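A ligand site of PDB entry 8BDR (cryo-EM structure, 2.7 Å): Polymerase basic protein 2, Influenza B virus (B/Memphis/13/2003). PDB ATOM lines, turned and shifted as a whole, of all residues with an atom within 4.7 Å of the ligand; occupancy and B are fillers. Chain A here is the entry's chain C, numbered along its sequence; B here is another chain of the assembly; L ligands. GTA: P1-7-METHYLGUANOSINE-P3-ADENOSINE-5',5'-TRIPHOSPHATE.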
ATOM      1  N   SER A 267      36.492  28.104 -25.544  1.00  0.00           N
ATOM      2  CA  SER A 267      35.356  28.688 -24.849  1.00  0.00           C
ATOM      3  C   SER A 267      35.411  28.395 -23.358  1.00  0.00           C
ATOM      4  O   SER A 267      35.225  29.294 -22.520  1.00  0.00           O
ATOM      5  CB  SER A 267      34.052  28.171 -25.450  1.00  0.00           C
ATOM      6  OG  SER A 267      32.923  28.760 -24.818  1.00  0.00           O
ATOM      7  N   GLN A 268      35.686  27.143 -22.996  1.00  0.00           N
ATOM      8  CA  GLN A 268      35.779  26.783 -21.592  1.00  0.00           C
ATOM      9  C   GLN A 268      36.913  27.531 -20.911  1.00  0.00           C
ATOM     10  O   GLN A 268      36.759  28.032 -19.791  1.00  0.00           O
ATOM     11  CB  GLN A 268      35.965  25.274 -21.452  1.00  0.00           C
ATOM     12  CG  GLN A 268      35.713  24.725 -20.053  1.00  0.00           C
ATOM     13  CD  GLN A 268      36.982  24.623 -19.218  1.00  0.00           C
ATOM     14  OE1 GLN A 268      38.093  24.801 -19.729  1.00  0.00           O
ATOM     15  NE2 GLN A 268      36.824  24.316 -17.939  1.00  0.00           N
ATOM     16  N   ILE A 271      35.939  31.145 -20.366  1.00  0.00           N
ATOM     17  CA  ILE A 271      34.966  31.240 -19.282  1.00  0.00           C
ATOM     18  C   ILE A 271      35.686  31.179 -17.933  1.00  0.00           C
ATOM     19  O   ILE A 271      35.422  31.980 -17.036  1.00  0.00           O
ATOM     20  CB  ILE A 271      33.909  30.129 -19.409  1.00  0.00           C
ATOM     21  CG1 ILE A 271      32.970  30.429 -20.584  1.00  0.00           C
ATOM     22  CG2 ILE A 271      33.110  30.002 -18.117  1.00  0.00           C
ATOM     23  CD1 ILE A 271      32.188  29.229 -21.056  1.00  0.00           C
ATOM     24  N   ARG A 275      35.893  34.219 -15.181  1.00  0.00           N
ATOM     25  CA  ARG A 275      35.443  34.013 -13.819  1.00  0.00           C
ATOM     26  C   ARG A 275      36.537  34.367 -12.819  1.00  0.00           C
ATOM     27  O   ARG A 275      36.287  35.048 -11.824  1.00  0.00           O
ATOM     28  CB  ARG A 275      34.987  32.559 -13.627  1.00  0.00           C
ATOM     29  CG  ARG A 275      33.628  32.258 -14.225  1.00  0.00           C
ATOM     30  CD  ARG A 275      33.180  30.845 -13.917  1.00  0.00           C
ATOM     31  NE  ARG A 275      31.904  30.530 -14.555  1.00  0.00           N
ATOM     32  CZ  ARG A 275      31.337  29.331 -14.530  1.00  0.00           C
ATOM     33  NH1 ARG A 275      31.902  28.304 -13.910  1.00  0.00           N
ATOM     34  NH2 ARG A 275      30.169  29.165 -15.146  1.00  0.00           N
ATOM     35  N   GLY A 314      29.706  32.890 -27.714  1.00  0.00           N
ATOM     36  CA  GLY A 314      29.184  32.203 -26.558  1.00  0.00           C
ATOM     37  C   GLY A 314      29.918  32.611 -25.300  1.00  0.00           C
ATOM     38  O   GLY A 314      30.771  33.511 -25.324  1.00  0.00           O
ATOM     39  N   GLY A 315      29.580  31.942 -24.203  1.00  0.00           N
ATOM     40  CA  GLY A 315      30.196  32.218 -22.921  1.00  0.00           C
ATOM     41  C   GLY A 315      29.224  32.137 -21.773  1.00  0.00           C
ATOM     42  O   GLY A 315      28.242  31.397 -21.828  1.00  0.00           O
ATOM     43  N   ASP A 316      29.488  32.907 -20.716  1.00  0.00           N
ATOM     44  CA  ASP A 316      28.634  32.944 -19.541  1.00  0.00           C
ATOM     45  C   ASP A 316      28.518  34.389 -19.075  1.00  0.00           C
ATOM     46  O   ASP A 316      28.889  35.318 -19.794  1.00  0.00           O
ATOM     47  CB  ASP A 316      29.190  32.012 -18.447  1.00  0.00           C
ATOM     48  CG  ASP A 316      30.246  32.682 -17.582  1.00  0.00           C
ATOM     49  OD1 ASP A 316      31.345  32.963 -18.091  1.00  0.00           O
ATOM     50  OD2 ASP A 316      29.966  32.938 -16.397  1.00  0.00           O
ATOM     51  N   ARG A 333      24.424  34.215 -24.630  1.00  0.00           N
ATOM     52  CA  ARG A 333      24.306  32.829 -25.059  1.00  0.00           C
ATOM     53  C   ARG A 333      24.667  31.890 -23.913  1.00  0.00           C
ATOM     54  O   ARG A 333      25.448  32.232 -23.021  1.00  0.00           O
ATOM     55  CB  ARG A 333      25.196  32.549 -26.266  1.00  0.00           C
ATOM     56  CG  ARG A 333      24.861  33.381 -27.489  1.00  0.00           C
ATOM     57  CD  ARG A 333      24.076  32.588 -28.527  1.00  0.00           C
ATOM     58  NE  ARG A 333      24.906  31.608 -29.215  1.00  0.00           N
ATOM     59  CZ  ARG A 333      24.968  30.320 -28.923  1.00  0.00           C
ATOM     60  NH1 ARG A 333      24.244  29.797 -27.944  1.00  0.00           N
ATOM     61  NH2 ARG A 333      25.766  29.526 -29.637  1.00  0.00           N
ATOM     62  N   GLN A 334      24.087  30.687 -23.947  1.00  0.00           N
ATOM     63  CA  GLN A 334      24.293  29.681 -22.919  1.00  0.00           C
ATOM     64  C   GLN A 334      24.294  28.311 -23.557  1.00  0.00           C
ATOM     65  O   GLN A 334      23.555  28.052 -24.522  1.00  0.00           O
ATOM     66  CB  GLN A 334      23.192  29.760 -21.850  1.00  0.00           C
ATOM     67  CG  GLN A 334      23.340  30.921 -20.894  1.00  0.00           C
ATOM     68  CD  GLN A 334      22.122  31.106 -20.016  1.00  0.00           C
ATOM     69  OE1 GLN A 334      21.338  30.185 -19.813  1.00  0.00           O
ATOM     70  NE2 GLN A 334      21.953  32.318 -19.480  1.00  0.00           N
ATOM     71  N   ARG A 335      25.121  27.426 -23.011  1.00  0.00           N
ATOM     72  CA  ARG A 335      25.251  26.051 -23.483  1.00  0.00           C
ATOM     73  C   ARG A 335      24.866  25.102 -22.362  1.00  0.00           C
ATOM     74  O   ARG A 335      25.291  25.285 -21.213  1.00  0.00           O
ATOM     75  CB  ARG A 335      26.687  25.763 -23.946  1.00  0.00           C
ATOM     76  CG  ARG A 335      26.799  24.566 -24.879  1.00  0.00           C
ATOM     77  CD  ARG A 335      27.881  24.750 -25.939  1.00  0.00           C
ATOM     78  NE  ARG A 335      29.171  24.225 -25.509  1.00  0.00           N
ATOM     79  CZ  ARG A 335      30.348  24.818 -25.727  1.00  0.00           C
ATOM     80  NH1 ARG A 335      30.440  25.959 -26.385  1.00  0.00           N
ATOM     81  NH2 ARG A 335      31.456  24.236 -25.264  1.00  0.00           N
ATOM     82  N   PHE A 336      24.060  24.094 -22.687  1.00  0.00           N
ATOM     83  CA  PHE A 336      23.629  23.073 -21.748  1.00  0.00           C
ATOM     84  C   PHE A 336      23.933  21.689 -22.310  1.00  0.00           C
ATOM     85  O   PHE A 336      23.093  20.790 -22.319  1.00  0.00           O
ATOM     86  CB  PHE A 336      22.153  23.224 -21.413  1.00  0.00           C
ATOM     87  CG  PHE A 336      21.657  22.262 -20.372  1.00  0.00           C
ATOM     88  CD1 PHE A 336      22.235  22.231 -19.113  1.00  0.00           C
ATOM     89  CD2 PHE A 336      20.605  21.404 -20.650  1.00  0.00           C
ATOM     90  CE1 PHE A 336      21.777  21.342 -18.155  1.00  0.00           C
ATOM     91  CE2 PHE A 336      20.148  20.525 -19.692  1.00  0.00           C
ATOM     92  CZ  PHE A 336      20.734  20.494 -18.444  1.00  0.00           C
ATOM     93  N   ARG A 343      19.253  34.409 -24.476  1.00  0.00           N
ATOM     94  CA  ARG A 343      18.301  35.127 -23.644  1.00  0.00           C
ATOM     95  C   ARG A 343      17.499  36.113 -24.484  1.00  0.00           C
ATOM     96  O   ARG A 343      18.025  36.731 -25.411  1.00  0.00           O
ATOM     97  CB  ARG A 343      19.030  35.858 -22.517  1.00  0.00           C
ATOM     98  CG  ARG A 343      18.126  36.665 -21.595  1.00  0.00           C
ATOM     99  CD  ARG A 343      17.287  35.785 -20.687  1.00  0.00           C
ATOM    100  NE  ARG A 343      18.088  34.763 -20.026  1.00  0.00           N
ATOM    101  CZ  ARG A 343      18.560  34.864 -18.782  1.00  0.00           C
ATOM    102  NH1 ARG A 343      18.333  35.935 -18.041  1.00  0.00           N
ATOM    103  NH2 ARG A 343      19.284  33.862 -18.287  1.00  0.00           N
ATOM    104  N   LYS A 350      20.141  31.722  -8.938  1.00  0.00           N
ATOM    105  CA  LYS A 350      20.422  30.336  -8.549  1.00  0.00           C
ATOM    106  C   LYS A 350      20.468  30.233  -7.027  1.00  0.00           C
ATOM    107  O   LYS A 350      21.166  30.993  -6.364  1.00  0.00           O
ATOM    108  CB  LYS A 350      21.743  29.878  -9.148  1.00  0.00           C
ATOM    109  CG  LYS A 350      21.987  28.379  -9.070  1.00  0.00           C
ATOM    110  CD  LYS A 350      23.342  28.016  -9.646  1.00  0.00           C
ATOM    111  CE  LYS A 350      23.610  26.524  -9.553  1.00  0.00           C
ATOM    112  NZ  LYS A 350      24.934  26.154 -10.123  1.00  0.00           N
ATOM    113  N   TRP A 368      16.797  27.583 -10.275  1.00  0.00           N
ATOM    114  CA  TRP A 368      16.734  28.948 -10.785  1.00  0.00           C
ATOM    115  C   TRP A 368      15.293  29.440 -10.732  1.00  0.00           C
ATOM    116  O   TRP A 368      14.378  28.765 -11.196  1.00  0.00           O
ATOM    117  CB  TRP A 368      17.260  29.012 -12.218  1.00  0.00           C
ATOM    118  CG  TRP A 368      18.722  28.724 -12.337  1.00  0.00           C
ATOM    119  CD1 TRP A 368      19.321  27.500 -12.330  1.00  0.00           C
ATOM    120  CD2 TRP A 368      19.774  29.678 -12.503  1.00  0.00           C
ATOM    121  NE1 TRP A 368      20.685  27.637 -12.479  1.00  0.00           N
ATOM    122  CE2 TRP A 368      20.988  28.967 -12.579  1.00  0.00           C
ATOM    123  CE3 TRP A 368      19.811  31.080 -12.579  1.00  0.00           C
ATOM    124  CZ2 TRP A 368      22.213  29.591 -12.732  1.00  0.00           C
ATOM    125  CZ3 TRP A 368      21.036  31.704 -12.731  1.00  0.00           C
ATOM    126  CH2 TRP A 368      22.218  30.966 -12.803  1.00  0.00           C
ATOM    127  N   GLU A 372      11.845  33.379 -17.482  1.00  0.00           N
ATOM    128  CA  GLU A 372      12.852  33.588 -18.513  1.00  0.00           C
ATOM    129  C   GLU A 372      12.310  33.170 -19.875  1.00  0.00           C
ATOM    130  O   GLU A 372      11.515  32.225 -19.991  1.00  0.00           O
ATOM    131  CB  GLU A 372      14.132  32.792 -18.221  1.00  0.00           C
ATOM    132  CG  GLU A 372      14.543  32.801 -16.757  1.00  0.00           C
ATOM    133  CD  GLU A 372      15.956  32.272 -16.560  1.00  0.00           C
ATOM    134  OE1 GLU A 372      16.864  32.718 -17.288  1.00  0.00           O
ATOM    135  OE2 GLU A 372      16.140  31.410 -15.677  1.00  0.00           O
ATOM    136  N   LYS A 387       9.959  29.807 -19.429  1.00  0.00           N
ATOM    137  CA  LYS A 387      10.253  29.042 -18.231  1.00  0.00           C
ATOM    138  C   LYS A 387       9.957  29.868 -16.986  1.00  0.00           C
ATOM    139  O   LYS A 387      10.154  31.088 -16.970  1.00  0.00           O
ATOM    140  CB  LYS A 387      11.717  28.574 -18.235  1.00  0.00           C
ATOM    141  CG  LYS A 387      12.259  28.086 -16.889  1.00  0.00           C
ATOM    142  CD  LYS A 387      13.186  29.110 -16.260  1.00  0.00           C
ATOM    143  CE  LYS A 387      13.514  28.776 -14.822  1.00  0.00           C
ATOM    144  NZ  LYS A 387      13.869  27.339 -14.639  1.00  0.00           N
ATOM    145  N   PHE A 415      16.044  21.178 -18.553  1.00  0.00           N
ATOM    146  CA  PHE A 415      16.614  22.491 -18.239  1.00  0.00           C
ATOM    147  C   PHE A 415      15.687  23.270 -17.314  1.00  0.00           C
ATOM    148  O   PHE A 415      16.152  23.940 -16.382  1.00  0.00           O
ATOM    149  CB  PHE A 415      16.881  23.253 -19.548  1.00  0.00           C
ATOM    150  CG  PHE A 415      17.378  24.674 -19.362  1.00  0.00           C
ATOM    151  CD1 PHE A 415      16.594  25.634 -18.738  1.00  0.00           C
ATOM    152  CD2 PHE A 415      18.607  25.064 -19.878  1.00  0.00           C
ATOM    153  CE1 PHE A 415      17.044  26.930 -18.585  1.00  0.00           C
ATOM    154  CE2 PHE A 415      19.057  26.360 -19.725  1.00  0.00           C
ATOM    155  CZ  PHE A 415      18.275  27.299 -19.083  1.00  0.00           C
ATOM    156  N   GLN A 417      13.940  22.402 -14.964  1.00  0.00           N
ATOM    157  CA  GLN A 417      13.903  21.904 -13.587  1.00  0.00           C
ATOM    158  C   GLN A 417      12.467  21.738 -13.107  1.00  0.00           C
ATOM    159  O   GLN A 417      12.153  21.987 -11.935  1.00  0.00           O
ATOM    160  CB  GLN A 417      14.695  22.816 -12.651  1.00  0.00           C
ATOM    161  CG  GLN A 417      16.153  23.004 -13.041  1.00  0.00           C
ATOM    162  CD  GLN A 417      16.852  24.030 -12.188  1.00  0.00           C
ATOM    163  OE1 GLN A 417      16.255  25.032 -11.795  1.00  0.00           O
ATOM    164  NE2 GLN A 417      18.124  23.789 -11.891  1.00  0.00           N
ATOM    165  N   SER A 440      27.955  17.640 -11.861  1.00  0.00           N
ATOM    166  CA  SER A 440      26.870  18.575 -12.110  1.00  0.00           C
ATOM    167  C   SER A 440      25.543  17.817 -12.184  1.00  0.00           C
ATOM    168  O   SER A 440      25.316  17.056 -13.125  1.00  0.00           O
ATOM    169  CB  SER A 440      27.111  19.349 -13.402  1.00  0.00           C
ATOM    170  OG  SER A 440      26.171  20.404 -13.547  1.00  0.00           O
ATOM    171  N   MET A 442      22.583  18.733 -13.046  1.00  0.00           N
ATOM    172  CA  MET A 442      21.794  19.029 -14.233  1.00  0.00           C
ATOM    173  C   MET A 442      22.267  18.212 -15.424  1.00  0.00           C
ATOM    174  O   MET A 442      21.454  17.640 -16.157  1.00  0.00           O
ATOM    175  CB  MET A 442      21.877  20.527 -14.546  1.00  0.00           C
ATOM    176  CG  MET A 442      21.054  21.396 -13.604  1.00  0.00           C
ATOM    177  SD  MET A 442      19.282  21.219 -13.885  1.00  0.00           S
ATOM    178  CE  MET A 442      18.817  20.224 -12.463  1.00  0.00           C
ATOM    179  N   TYR A 443      23.581  18.137 -15.634  1.00  0.00           N
ATOM    180  CA  TYR A 443      24.092  17.373 -16.765  1.00  0.00           C
ATOM    181  C   TYR A 443      23.871  15.877 -16.566  1.00  0.00           C
ATOM    182  O   TYR A 443      23.609  15.151 -17.536  1.00  0.00           O
ATOM    183  CB  TYR A 443      25.578  17.675 -16.975  1.00  0.00           C
ATOM    184  CG  TYR A 443      25.834  18.987 -17.694  1.00  0.00           C
ATOM    185  CD1 TYR A 443      25.924  20.173 -17.000  1.00  0.00           C
ATOM    186  CD2 TYR A 443      26.000  19.019 -19.073  1.00  0.00           C
ATOM    187  CE1 TYR A 443      26.168  21.370 -17.645  1.00  0.00           C
ATOM    188  CE2 TYR A 443      26.238  20.207 -19.738  1.00  0.00           C
ATOM    189  CZ  TYR A 443      26.324  21.382 -19.014  1.00  0.00           C
ATOM    190  OH  TYR A 443      26.564  22.569 -19.669  1.00  0.00           O
ATOM    191  N   SER A 529      29.123  32.483 -11.386  1.00  0.00           N
ATOM    192  CA  SER A 529      29.195  31.257 -10.607  1.00  0.00           C
ATOM    193  C   SER A 529      30.482  31.206  -9.802  1.00  0.00           C
ATOM    194  O   SER A 529      31.526  31.706 -10.215  1.00  0.00           O
ATOM    195  CB  SER A 529      29.112  30.038 -11.532  1.00  0.00           C
ATOM    196  OG  SER A 529      29.219  28.831 -10.789  1.00  0.00           O
ATOM    197  N   LEU A 531      31.857  28.298  -8.885  1.00  0.00           N
ATOM    198  CA  LEU A 531      32.521  27.015  -9.114  1.00  0.00           C
ATOM    199  C   LEU A 531      33.948  27.244  -9.606  1.00  0.00           C
ATOM    200  O   LEU A 531      34.181  28.057 -10.492  1.00  0.00           O
ATOM    201  CB  LEU A 531      31.738  26.180 -10.126  1.00  0.00           C
ATOM    202  CG  LEU A 531      32.301  24.789 -10.405  1.00  0.00           C
ATOM    203  CD1 LEU A 531      31.935  23.830  -9.289  1.00  0.00           C
ATOM    204  CD2 LEU A 531      31.816  24.264 -11.749  1.00  0.00           C
ATOM    205  P     A B   1      33.157  22.592 -16.943  1.00  0.00           P
ATOM    206  OP1   A B   1      33.836  23.480 -15.955  1.00  0.00           O
ATOM    207  OP2   A B   1      33.953  22.032 -18.065  1.00  0.00           O
ATOM    208  O5'   A B   1      32.486  21.393 -16.144  1.00  0.00           O
ATOM    209  C5'   A B   1      32.772  20.044 -16.483  1.00  0.00           C
ATOM    210  C4'   A B   1      31.626  19.133 -16.108  1.00  0.00           C
ATOM    211  O4'   A B   1      30.418  19.559 -16.781  1.00  0.00           O
ATOM    212  C3'   A B   1      31.783  17.670 -16.522  1.00  0.00           C
ATOM    213  O3'   A B   1      32.575  16.922 -15.626  1.00  0.00           O
ATOM    214  C2'   A B   1      30.334  17.195 -16.594  1.00  0.00           C
ATOM    215  O2'   A B   1      29.831  16.899 -15.301  1.00  0.00           O
ATOM    216  C1'   A B   1      29.629  18.441 -17.131  1.00  0.00           C
ATOM    217  N9    A B   1      29.475  18.418 -18.590  1.00  0.00           N
ATOM    218  C8    A B   1      29.992  19.298 -19.510  1.00  0.00           C
ATOM    219  N7    A B   1      29.672  19.022 -20.753  1.00  0.00           N
ATOM    220  C5    A B   1      28.901  17.876 -20.647  1.00  0.00           C
ATOM    221  C6    A B   1      28.257  17.074 -21.604  1.00  0.00           C
ATOM    222  N6    A B   1      28.299  17.314 -22.915  1.00  0.00           N
ATOM    223  N1    A B   1      27.564  15.996 -21.169  1.00  0.00           N
ATOM    224  C2    A B   1      27.524  15.755 -19.847  1.00  0.00           C
ATOM    225  N3    A B   1      28.085  16.432 -18.854  1.00  0.00           N
ATOM    226  C4    A B   1      28.769  17.493 -19.320  1.00  0.00           C
HETATM  227  N2  GTA L   1      20.269  32.168 -16.076  1.00  0.00           N
HETATM  228  O6  GTA L   1      17.616  28.491 -15.132  1.00  0.00           O
HETATM  229  C6  GTA L   1      18.661  28.964 -15.580  1.00  0.00           C
HETATM  230  C5  GTA L   1      19.607  28.170 -16.089  1.00  0.00           C
HETATM  231  N7  GTA L   1      19.683  26.844 -16.225  1.00  0.00           N
HETATM  232  C7  GTA L   1      18.667  25.840 -15.837  1.00  0.00           C
HETATM  233  C8  GTA L   1      20.848  26.549 -16.795  1.00  0.00           C
HETATM  234  N9  GTA L   1      21.494  27.684 -16.998  1.00  0.00           N
HETATM  235  C4  GTA L   1      20.740  28.688 -16.572  1.00  0.00           C
HETATM  236  N3  GTA L   1      20.965  30.016 -16.562  1.00  0.00           N
HETATM  237  C2  GTA L   1      20.048  30.858 -16.075  1.00  0.00           C
HETATM  238  N1  GTA L   1      18.861  30.344 -15.560  1.00  0.00           N
HETATM  239  O3A GTA L   1      24.882  28.874 -18.829  1.00  0.00           O
HETATM  240  C1A GTA L   1      22.844  27.809 -17.618  1.00  0.00           C
HETATM  241  C2A GTA L   1      23.861  28.469 -16.694  1.00  0.00           C
HETATM  242  C3A GTA L   1      25.050  28.207 -17.584  1.00  0.00           C
HETATM  243  C4A GTA L   1      24.894  26.695 -17.771  1.00  0.00           C
HETATM  244  C5A GTA L   1      25.308  25.895 -16.531  1.00  0.00           C
HETATM  245  O4A GTA L   1      23.455  26.509 -17.940  1.00  0.00           O
HETATM  246  O2A GTA L   1      23.606  29.868 -16.512  1.00  0.00           O
HETATM  247  P1  GTA L   1      24.423  25.058 -14.191  1.00  0.00           P
HETATM  248  O11 GTA L   1      25.542  24.106 -14.290  1.00  0.00           O
HETATM  249  O12 GTA L   1      23.094  24.564 -13.766  1.00  0.00           O
HETATM  250  O13 GTA L   1      24.843  26.250 -13.178  1.00  0.00           O
HETATM  251  O15 GTA L   1      24.240  25.829 -15.586  1.00  0.00           O
HETATM  252  P2  GTA L   1      26.218  27.085 -13.373  1.00  0.00           P
HETATM  253  O22 GTA L   1      26.720  27.437 -12.029  1.00  0.00           O
HETATM  254  O21 GTA L   1      26.010  28.139 -14.376  1.00  0.00           O
HETATM  255  O23 GTA L   1      27.220  25.982 -13.987  1.00  0.00           O
HETATM  256  P3  GTA L   1      28.724  25.870 -13.429  1.00  0.00           P
HETATM  257  O32 GTA L   1      29.346  27.207 -13.484  1.00  0.00           O
HETATM  258  O31 GTA L   1      28.686  25.130 -12.158  1.00  0.00           O
HETATM  259  O33 GTA L   1      29.432  24.945 -14.547  1.00  0.00           O
HETATM  260  C5B GTA L   1      28.815  24.790 -15.827  1.00  0.00           C
HETATM  261  C4B GTA L   1      29.693  23.915 -16.751  1.00  0.00           C
HETATM  262  O4B GTA L   1      29.223  24.186 -18.113  1.00  0.00           O
HETATM  263  C3B GTA L   1      31.163  24.326 -16.793  1.00  0.00           C
HETATM  264  O3B GTA L   1      31.925  23.390 -17.574  1.00  0.00           O
HETATM  265  C2B GTA L   1      31.017  25.608 -17.550  1.00  0.00           C
HETATM  266  O2B GTA L   1      32.288  26.165 -17.935  1.00  0.00           O
HETATM  267  C1B GTA L   1      30.265  25.025 -18.740  1.00  0.00           C
HETATM  268  N9C GTA L   1      29.714  26.082 -19.626  1.00  0.00           N
HETATM  269  C8C GTA L   1      28.736  26.910 -19.271  1.00  0.00           C
HETATM  270  N7C GTA L   1      28.503  27.718 -20.303  1.00  0.00           N
HETATM  271  C5C GTA L   1      29.337  27.385 -21.287  1.00  0.00           C
HETATM  272  C6C GTA L   1      29.490  27.890 -22.515  1.00  0.00           C
HETATM  273  N6C GTA L   1      28.684  28.905 -22.826  1.00  0.00           N
HETATM  274  N1C GTA L   1      30.394  27.409 -23.365  1.00  0.00           N
HETATM  275  C2C GTA L   1      31.197  26.346 -22.954  1.00  0.00           C
HETATM  276  N3C GTA L   1      31.015  25.829 -21.670  1.00  0.00           N
HETATM  277  C4C GTA L   1      30.084  26.377 -20.870  1.00  0.00           C
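N1C of the ligand sits at hydrogen-bond distance from OG of Ser 267, 3.2 Å away. P of A 1 of chain B is covalently linked to an oxygen (O3B) of the ligand, at 1.6 Å. An oxygen (O4B) of the ligand is in hydrogen-bond range of the side-chain hydroxyl of Tyr 443 (3.5 Å). The side-chain carboxylate (OE2) of Glu 372 is in hydrogen-bond range of a nitrogen (N1) of the ligand, at 2.9 Å. The side-chain hydroxyl (OG) of Ser 529 lies within hydrogen-bond range of an oxygen (O22) of the ligand. NH1 of Arg 335 sits at hydrogen-bond distance from N1C of the ligand. The guanidinium group (NH2) of Arg 275 is in salt-bridge range of an oxygen (O32) of the ligand, 2.7 Å away. The side-chain amino group (NZ) of Lys 350 is in salt-bridge range of an oxygen (O22) of the ligand (2.9 Å). A nitrogen (N3) of the ligand lies close to the side-chain amide oxygen of Gln 334. A nitrogen (N6C) of the ligand is in hydrogen-bond range of the backbone carbonyl oxygen of Gly 315, 2.7 Å away.
N of Trp 368 lies within hydrogen-bond range of OE1 of Gln 417 (3.0 Å). The side-chain hydroxyl of Ser 529 sits at hydrogen-bond distance from the backbone NH of Leu 531, at 3.3 Å. The side-chain carboxylate (OD2) of Asp 316 lies within salt-bridge range of the guanidinium group (NE) of Arg 275 (3.6 Å). OE1 of Glu 372 is in salt-bridge range of NH2 of Arg 343 (2.9 Å). The side-chain sulfur (SD) of Met 442 is in hydrogen-bond range of the side-chain amide nitrogen (NE2) of Gln 417. The guanidinium group (NH2) of Arg 343 sits close to the side-chain amide nitrogen (NE2) of Gln 334, at 3.3 Å. The backbone carbonyl oxygen of Lys 387 lies within hydrogen-bond range of the backbone NH of Glu 372, 2.9 Å away. The backbone carbonyl oxygen (O) of Arg 335 lies within hydrogen-bond range of the side-chain hydroxyl (OH) of Tyr 443, 3.4 Å away.
NH2 of Arg 343 sits close to N2 of the ligand. Ile 271 touches the ligand. Trp 368 touches the ligand (CB to O6, 3.0 Å). Lys 387 touches the ligand (NZ to O6, 3.95 Å). Phe 415 touches the ligand. Ser 440 touches the ligand. Met 442 touches the ligand (CG to O12, 3.8 Å). Leu 531 touches the ligand. Hydrophobic or aromatic side chains that line the ligand: Ile 271, Trp 368, Phe 415, Met 442 and Leu 531. 18 residues have an atom within 4 Å of the ligand: Ser 267, Ile 271, Arg 275, Gly 315, Gln 334, Arg 335, Arg 343, Lys 350, Trp 368, Glu 372, Lys 387, Phe 415, Ser 440, Met 442, Tyr 443, Ser 529, Leu 531 and A 1 of chain B. The nearest printed residue that does not touch the ligand is Gln 268 (4.3 Å).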
